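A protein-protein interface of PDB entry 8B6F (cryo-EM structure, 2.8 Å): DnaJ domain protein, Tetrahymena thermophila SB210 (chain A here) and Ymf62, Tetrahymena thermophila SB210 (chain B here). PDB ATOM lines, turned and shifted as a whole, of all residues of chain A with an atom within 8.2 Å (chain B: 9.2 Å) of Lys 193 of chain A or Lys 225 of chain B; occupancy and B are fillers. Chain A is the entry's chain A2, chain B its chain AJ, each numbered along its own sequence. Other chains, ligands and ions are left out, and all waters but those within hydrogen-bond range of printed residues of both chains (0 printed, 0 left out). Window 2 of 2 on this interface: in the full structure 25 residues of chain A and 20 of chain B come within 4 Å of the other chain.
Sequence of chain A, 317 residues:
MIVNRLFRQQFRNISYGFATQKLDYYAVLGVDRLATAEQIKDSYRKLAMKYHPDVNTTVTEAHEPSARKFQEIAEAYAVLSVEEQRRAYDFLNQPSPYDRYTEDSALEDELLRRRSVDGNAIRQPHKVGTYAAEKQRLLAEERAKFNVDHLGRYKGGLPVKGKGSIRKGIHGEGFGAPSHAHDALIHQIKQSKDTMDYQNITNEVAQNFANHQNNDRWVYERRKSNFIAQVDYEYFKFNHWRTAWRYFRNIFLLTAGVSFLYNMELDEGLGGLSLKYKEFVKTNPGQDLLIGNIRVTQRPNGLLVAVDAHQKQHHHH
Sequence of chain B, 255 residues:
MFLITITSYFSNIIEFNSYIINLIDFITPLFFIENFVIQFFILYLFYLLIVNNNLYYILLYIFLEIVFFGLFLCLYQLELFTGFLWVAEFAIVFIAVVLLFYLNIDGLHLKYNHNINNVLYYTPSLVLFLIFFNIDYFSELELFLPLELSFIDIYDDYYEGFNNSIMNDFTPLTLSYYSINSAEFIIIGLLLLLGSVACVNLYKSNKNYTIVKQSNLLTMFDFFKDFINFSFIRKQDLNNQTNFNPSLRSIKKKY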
ATOM      1  N   ILE A 186       6.366 -13.508   4.840  1.00  0.00           N
ATOM      2  CA  ILE A 186       6.452 -13.158   6.254  1.00  0.00           C
ATOM      3  C   ILE A 186       5.266 -12.288   6.650  1.00  0.00           C
ATOM      4  O   ILE A 186       4.686 -12.457   7.729  1.00  0.00           O
ATOM      5  CB  ILE A 186       7.793 -12.461   6.551  1.00  0.00           C
ATOM      6  CG1 ILE A 186       8.973 -13.360   6.167  1.00  0.00           C
ATOM      7  CG2 ILE A 186       7.884 -12.067   8.019  1.00  0.00           C
ATOM      8  CD1 ILE A 186       9.031 -14.678   6.909  1.00  0.00           C
ATOM      9  N   HIS A 187       4.888 -11.345   5.788  1.00  0.00           N
ATOM     10  CA  HIS A 187       3.717 -10.522   6.069  1.00  0.00           C
ATOM     11  C   HIS A 187       2.473 -11.384   6.231  1.00  0.00           C
ATOM     12  O   HIS A 187       1.678 -11.176   7.155  1.00  0.00           O
ATOM     13  CB  HIS A 187       3.518  -9.497   4.953  1.00  0.00           C
ATOM     14  CG  HIS A 187       2.367  -8.566   5.182  1.00  0.00           C
ATOM     15  ND1 HIS A 187       2.533  -7.244   5.532  1.00  0.00           N
ATOM     16  CD2 HIS A 187       1.031  -8.767   5.106  1.00  0.00           C
ATOM     17  CE1 HIS A 187       1.351  -6.672   5.664  1.00  0.00           C
ATOM     18  NE2 HIS A 187       0.421  -7.575   5.410  1.00  0.00           N
ATOM     19  N   GLN A 188       2.283 -12.356   5.339  1.00  0.00           N
ATOM     20  CA  GLN A 188       1.119 -13.229   5.433  1.00  0.00           C
ATOM     21  C   GLN A 188       1.157 -14.061   6.707  1.00  0.00           C
ATOM     22  O   GLN A 188       0.132 -14.232   7.375  1.00  0.00           O
ATOM     23  CB  GLN A 188       1.046 -14.135   4.205  1.00  0.00           C
ATOM     24  CG  GLN A 188      -0.196 -15.006   4.156  1.00  0.00           C
ATOM     25  CD  GLN A 188      -0.185 -15.968   2.988  1.00  0.00           C
ATOM     26  OE1 GLN A 188       0.809 -16.084   2.274  1.00  0.00           O
ATOM     27  NE2 GLN A 188      -1.296 -16.668   2.787  1.00  0.00           N
ATOM     28  N   ILE A 189       2.328 -14.596   7.056  1.00  0.00           N
ATOM     29  CA  ILE A 189       2.441 -15.398   8.272  1.00  0.00           C
ATOM     30  C   ILE A 189       2.085 -14.563   9.494  1.00  0.00           C
ATOM     31  O   ILE A 189       1.378 -15.027  10.395  1.00  0.00           O
ATOM     32  CB  ILE A 189       3.858 -15.995   8.384  1.00  0.00           C
ATOM     33  CG1 ILE A 189       4.054 -17.084   7.329  1.00  0.00           C
ATOM     34  CG2 ILE A 189       4.103 -16.558   9.782  1.00  0.00           C
ATOM     35  CD1 ILE A 189       5.472 -17.611   7.240  1.00  0.00           C
ATOM     36  N   LYS A 190       2.568 -13.321   9.550  1.00  0.00           N
ATOM     37  CA  LYS A 190       2.289 -12.477  10.707  1.00  0.00           C
ATOM     38  C   LYS A 190       0.816 -12.095  10.771  1.00  0.00           C
ATOM     39  O   LYS A 190       0.177 -12.222  11.821  1.00  0.00           O
ATOM     40  CB  LYS A 190       3.165 -11.224  10.664  1.00  0.00           C
ATOM     41  CG  LYS A 190       4.651 -11.485  10.874  1.00  0.00           C
ATOM     42  CD  LYS A 190       4.971 -11.968  12.285  1.00  0.00           C
ATOM     43  CE  LYS A 190       4.676 -10.906  13.331  1.00  0.00           C
ATOM     44  NZ  LYS A 190       5.164 -11.308  14.681  1.00  0.00           N
ATOM     45  N   GLN A 191       0.258 -11.620   9.655  1.00  0.00           N
ATOM     46  CA  GLN A 191      -1.093 -11.068   9.684  1.00  0.00           C
ATOM     47  C   GLN A 191      -2.150 -12.162   9.778  1.00  0.00           C
ATOM     48  O   GLN A 191      -3.094 -12.046  10.565  1.00  0.00           O
ATOM     49  CB  GLN A 191      -1.332 -10.202   8.446  1.00  0.00           C
ATOM     50  CG  GLN A 191      -2.646  -9.431   8.487  1.00  0.00           C
ATOM     51  CD  GLN A 191      -2.824  -8.510   7.296  1.00  0.00           C
ATOM     52  OE1 GLN A 191      -2.001  -8.489   6.382  1.00  0.00           O
ATOM     53  NE2 GLN A 191      -3.905  -7.738   7.303  1.00  0.00           N
ATOM     54  N   SER A 192      -2.010 -13.225   8.992  1.00  0.00           N
ATOM     55  CA  SER A 192      -3.006 -14.285   8.889  1.00  0.00           C
ATOM     56  C   SER A 192      -2.440 -15.607   9.381  1.00  0.00           C
ATOM     57  O   SER A 192      -2.620 -16.653   8.755  1.00  0.00           O
ATOM     58  CB  SER A 192      -3.504 -14.427   7.452  1.00  0.00           C
ATOM     59  OG  SER A 192      -4.107 -13.228   6.996  1.00  0.00           O
ATOM     60  N   LYS A 193      -1.735 -15.571  10.508  1.00  0.00           N
ATOM     61  CA  LYS A 193      -1.102 -16.768  11.044  1.00  0.00           C
ATOM     62  C   LYS A 193      -2.104 -17.905  11.173  1.00  0.00           C
ATOM     63  O   LYS A 193      -3.167 -17.747  11.779  1.00  0.00           O
ATOM     64  CB  LYS A 193      -0.485 -16.460  12.410  1.00  0.00           C
ATOM     65  CG  LYS A 193      -1.461 -15.859  13.410  1.00  0.00           C
ATOM     66  CD  LYS A 193      -0.890 -14.600  14.041  1.00  0.00           C
ATOM     67  CE  LYS A 193      -1.889 -13.936  14.969  1.00  0.00           C
ATOM     68  NZ  LYS A 193      -3.095 -13.451  14.243  1.00  0.00           N
ATOM     69  N   ASP A 194      -1.755 -19.053  10.599  1.00  0.00           N
ATOM     70  CA  ASP A 194      -2.476 -20.323  10.665  1.00  0.00           C
ATOM     71  C   ASP A 194      -3.720 -20.354   9.782  1.00  0.00           C
ATOM     72  O   ASP A 194      -4.346 -21.412   9.683  1.00  0.00           O
ATOM     73  CB  ASP A 194      -2.880 -20.692  12.104  1.00  0.00           C
ATOM     74  CG  ASP A 194      -4.364 -20.506  12.374  1.00  0.00           C
ATOM     75  OD1 ASP A 194      -4.905 -19.414  12.103  1.00  0.00           O
ATOM     76  OD2 ASP A 194      -4.997 -21.462  12.868  1.00  0.00           O
ATOM     77  N   THR A 195      -4.090 -19.257   9.128  1.00  0.00           N
ATOM     78  CA  THR A 195      -5.305 -19.187   8.326  1.00  0.00           C
ATOM     79  C   THR A 195      -4.949 -19.091   6.849  1.00  0.00           C
ATOM     80  O   THR A 195      -4.161 -18.228   6.451  1.00  0.00           O
ATOM     81  CB  THR A 195      -6.161 -17.987   8.735  1.00  0.00           C
ATOM     82  OG1 THR A 195      -6.519 -18.101  10.118  1.00  0.00           O
ATOM     83  CG2 THR A 195      -7.431 -17.914   7.896  1.00  0.00           C
ATOM     84  N   MET A 196      -5.531 -19.979   6.045  1.00  0.00           N
ATOM     85  CA  MET A 196      -5.374 -19.952   4.592  1.00  0.00           C
ATOM     86  C   MET A 196      -6.723 -20.283   3.970  1.00  0.00           C
ATOM     87  O   MET A 196      -7.174 -21.429   4.041  1.00  0.00           O
ATOM     88  CB  MET A 196      -4.309 -20.941   4.120  1.00  0.00           C
ATOM     89  CG  MET A 196      -2.882 -20.497   4.388  1.00  0.00           C
ATOM     90  SD  MET A 196      -1.653 -21.634   3.715  1.00  0.00           S
ATOM     91  CE  MET A 196      -1.965 -21.496   1.958  1.00  0.00           C
ATOM     92  N   PHE B 221       9.118 -13.405  16.115  1.00  0.00           N
ATOM     93  CA  PHE B 221       7.788 -13.992  16.186  1.00  0.00           C
ATOM     94  C   PHE B 221       7.405 -14.220  17.640  1.00  0.00           C
ATOM     95  O   PHE B 221       8.197 -14.762  18.418  1.00  0.00           O
ATOM     96  CB  PHE B 221       7.730 -15.311  15.411  1.00  0.00           C
ATOM     97  CG  PHE B 221       7.865 -15.142  13.926  1.00  0.00           C
ATOM     98  CD1 PHE B 221       6.745 -14.948  13.135  1.00  0.00           C
ATOM     99  CD2 PHE B 221       9.110 -15.170  13.324  1.00  0.00           C
ATOM    100  CE1 PHE B 221       6.866 -14.788  11.769  1.00  0.00           C
ATOM    101  CE2 PHE B 221       9.240 -15.010  11.958  1.00  0.00           C
ATOM    102  CZ  PHE B 221       8.115 -14.819  11.179  1.00  0.00           C
ATOM    103  N   ASP B 222       6.194 -13.805  18.001  1.00  0.00           N
ATOM    104  CA  ASP B 222       5.703 -14.014  19.356  1.00  0.00           C
ATOM    105  C   ASP B 222       5.424 -15.493  19.585  1.00  0.00           C
ATOM    106  O   ASP B 222       4.705 -16.126  18.808  1.00  0.00           O
ATOM    107  CB  ASP B 222       4.436 -13.195  19.592  1.00  0.00           C
ATOM    108  CG  ASP B 222       4.646 -11.716  19.345  1.00  0.00           C
ATOM    109  OD1 ASP B 222       5.776 -11.229  19.557  1.00  0.00           O
ATOM    110  OD2 ASP B 222       3.680 -11.040  18.934  1.00  0.00           O
ATOM    111  N   PHE B 223       5.990 -16.044  20.657  1.00  0.00           N
ATOM    112  CA  PHE B 223       5.824 -17.466  20.923  1.00  0.00           C
ATOM    113  C   PHE B 223       4.400 -17.816  21.326  1.00  0.00           C
ATOM    114  O   PHE B 223       4.004 -18.980  21.203  1.00  0.00           O
ATOM    115  CB  PHE B 223       6.797 -17.914  22.012  1.00  0.00           C
ATOM    116  CG  PHE B 223       6.799 -19.394  22.244  1.00  0.00           C
ATOM    117  CD1 PHE B 223       7.311 -20.253  21.288  1.00  0.00           C
ATOM    118  CD2 PHE B 223       6.297 -19.927  23.418  1.00  0.00           C
ATOM    119  CE1 PHE B 223       7.316 -21.618  21.493  1.00  0.00           C
ATOM    120  CE2 PHE B 223       6.301 -21.292  23.632  1.00  0.00           C
ATOM    121  CZ  PHE B 223       6.812 -22.138  22.668  1.00  0.00           C
ATOM    122  N   PHE B 224       3.621 -16.844  21.792  1.00  0.00           N
ATOM    123  CA  PHE B 224       2.257 -17.077  22.249  1.00  0.00           C
ATOM    124  C   PHE B 224       1.201 -16.549  21.293  1.00  0.00           C
ATOM    125  O   PHE B 224       0.203 -17.228  21.053  1.00  0.00           O
ATOM    126  CB  PHE B 224       2.050 -16.439  23.628  1.00  0.00           C
ATOM    127  CG  PHE B 224       3.136 -16.768  24.610  1.00  0.00           C
ATOM    128  CD1 PHE B 224       3.260 -18.048  25.124  1.00  0.00           C
ATOM    129  CD2 PHE B 224       4.031 -15.794  25.023  1.00  0.00           C
ATOM    130  CE1 PHE B 224       4.259 -18.353  26.027  1.00  0.00           C
ATOM    131  CE2 PHE B 224       5.033 -16.092  25.925  1.00  0.00           C
ATOM    132  CZ  PHE B 224       5.146 -17.375  26.429  1.00  0.00           C
ATOM    133  N   LYS B 225       1.383 -15.346  20.748  1.00  0.00           N
ATOM    134  CA  LYS B 225       0.388 -14.798  19.834  1.00  0.00           C
ATOM    135  C   LYS B 225       0.454 -15.473  18.469  1.00  0.00           C
ATOM    136  O   LYS B 225      -0.584 -15.786  17.877  1.00  0.00           O
ATOM    137  CB  LYS B 225       0.578 -13.289  19.695  1.00  0.00           C
ATOM    138  CG  LYS B 225       0.349 -12.526  20.990  1.00  0.00           C
ATOM    139  CD  LYS B 225      -0.495 -11.279  20.770  1.00  0.00           C
ATOM    140  CE  LYS B 225      -1.953 -11.629  20.489  1.00  0.00           C
ATOM    141  NZ  LYS B 225      -2.805 -10.416  20.338  1.00  0.00           N
ATOM    142  N   ASP B 226       1.657 -15.706  17.954  1.00  0.00           N
ATOM    143  CA  ASP B 226       1.828 -16.287  16.630  1.00  0.00           C
ATOM    144  C   ASP B 226       1.854 -17.808  16.714  1.00  0.00           C
ATOM    145  O   ASP B 226       2.438 -18.383  17.636  1.00  0.00           O
ATOM    146  CB  ASP B 226       3.116 -15.781  15.976  1.00  0.00           C
ATOM    147  CG  ASP B 226       3.089 -14.288  15.721  1.00  0.00           C
ATOM    148  OD1 ASP B 226       2.006 -13.755  15.404  1.00  0.00           O
ATOM    149  OD2 ASP B 226       4.152 -13.645  15.837  1.00  0.00           O
ATOM    150  N   PHE B 227       1.219 -18.452  15.738  1.00  0.00           N
ATOM    151  CA  PHE B 227       1.106 -19.909  15.697  1.00  0.00           C
ATOM    152  C   PHE B 227       2.267 -20.442  14.868  1.00  0.00           C
ATOM    153  O   PHE B 227       2.202 -20.520  13.642  1.00  0.00           O
ATOM    154  CB  PHE B 227      -0.246 -20.320  15.124  1.00  0.00           C
ATOM    155  CG  PHE B 227      -0.508 -21.796  15.182  1.00  0.00           C
ATOM    156  CD1 PHE B 227      -0.551 -22.459  16.397  1.00  0.00           C
ATOM    157  CD2 PHE B 227      -0.745 -22.514  14.024  1.00  0.00           C
ATOM    158  CE1 PHE B 227      -0.805 -23.814  16.453  1.00  0.00           C
ATOM    159  CE2 PHE B 227      -0.999 -23.871  14.074  1.00  0.00           C
ATOM    160  CZ  PHE B 227      -1.029 -24.522  15.290  1.00  0.00           C
ATOM    161  N   ILE B 228       3.346 -20.817  15.551  1.00  0.00           N
ATOM    162  CA  ILE B 228       4.568 -21.297  14.915  1.00  0.00           C
ATOM    163  C   ILE B 228       4.653 -22.803  15.110  1.00  0.00           C
ATOM    164  O   ILE B 228       4.447 -23.306  16.219  1.00  0.00           O
ATOM    165  CB  ILE B 228       5.817 -20.596  15.478  1.00  0.00           C
ATOM    166  CG1 ILE B 228       5.952 -20.865  16.981  1.00  0.00           C
ATOM    167  CG2 ILE B 228       5.747 -19.101  15.185  1.00  0.00           C
ATOM    168  CD1 ILE B 228       7.112 -20.150  17.643  1.00  0.00           C
ATOM    169  N   ASN B 229       4.947 -23.520  14.030  1.00  0.00           N
ATOM    170  CA  ASN B 229       5.069 -24.967  14.088  1.00  0.00           C
ATOM    171  C   ASN B 229       6.398 -25.365  14.713  1.00  0.00           C
ATOM    172  O   ASN B 229       7.437 -24.759  14.441  1.00  0.00           O
ATOM    173  CB  ASN B 229       4.954 -25.565  12.686  1.00  0.00           C
ATOM    174  CG  ASN B 229       5.080 -27.072  12.687  1.00  0.00           C
ATOM    175  OD1 ASN B 229       4.809 -27.728  13.691  1.00  0.00           O
ATOM    176  ND2 ASN B 229       5.495 -27.632  11.558  1.00  0.00           N
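OD2 of Asp 226 of chain B is in salt-bridge range of NZ of Lys 190 of chain A, 2.8 Å away.
OD1 of Asp 194 of chain A sits at hydrogen-bond distance from OG1 of Thr 195 of chain A (2.9 Å).
N of Asp 222 of chain B is in hydrogen-bond range of OD2 of Asp 226 of chain B, at 3.0 Å.
Ile 189 of chain A touches Phe 221 of chain B (CG2 to CE1, 3.8 Å).
CD of Lys 190 of chain A touches CE1 of Phe 221 of chain B, at 3.4 Å.
Lys 193 of chain A touches Lys 225 of chain B.
OD1 of Asp 226 of chain B touches CD of Lys 193 of chain A, 3.3 Å away.
CB of Asp 194 of chain A touches CD2 of Phe 227 of chain B (3.4 Å).
Of the printed residues of chain B, Ile 189 of chain A touches Phe 221.
Of the printed residues of chain B, Lys 190 of chain A touches Phe 221 (3.4 Å) and Asp 226 (2.8 Å).
No residue of chain B comes within 4 Å of Ser 192 of chain A.
Of chain B, only Lys 225 (3.7 Å) and Asp 226 (3.3 Å) come within 4 Å of Lys 193 of chain A.
Of chain B, only Phe 227 (3.4 Å) comes within 4 Å of Asp 194 of chain A.
Printed residues of chain A within 4 Å of Phe 221 of chain B: Ile 189 and Lys 190.
Lys 225 of chain B touches just one residue of chain A: Lys 193 (3.7 Å).
Of the printed residues of chain A, Asp 226 of chain B touches Lys 190 and Lys 193.
Of the printed residues of chain A, Phe 227 of chain B touches Asp 194 (3.4 Å).
The nearest residue of chain B that does not touch Lys 193 of chain A is Phe 227 of chain B (4.2 Å).
Printed residues of chain A that touch a printed residue of chain B: Ile 189, Lys 190, Lys 193 and Asp 194.
Hydrophobic or aromatic side chains of chain B within 4 Å of the printed part of chain A: Phe 221 and Phe 227.
Among the printed residues, Asp or Glu carboxylates within 4 Å of a Lys or Arg side-chain nitrogen of the other chain: Lys 190 of chain A with Asp 226 of chain B (2.8 Å).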
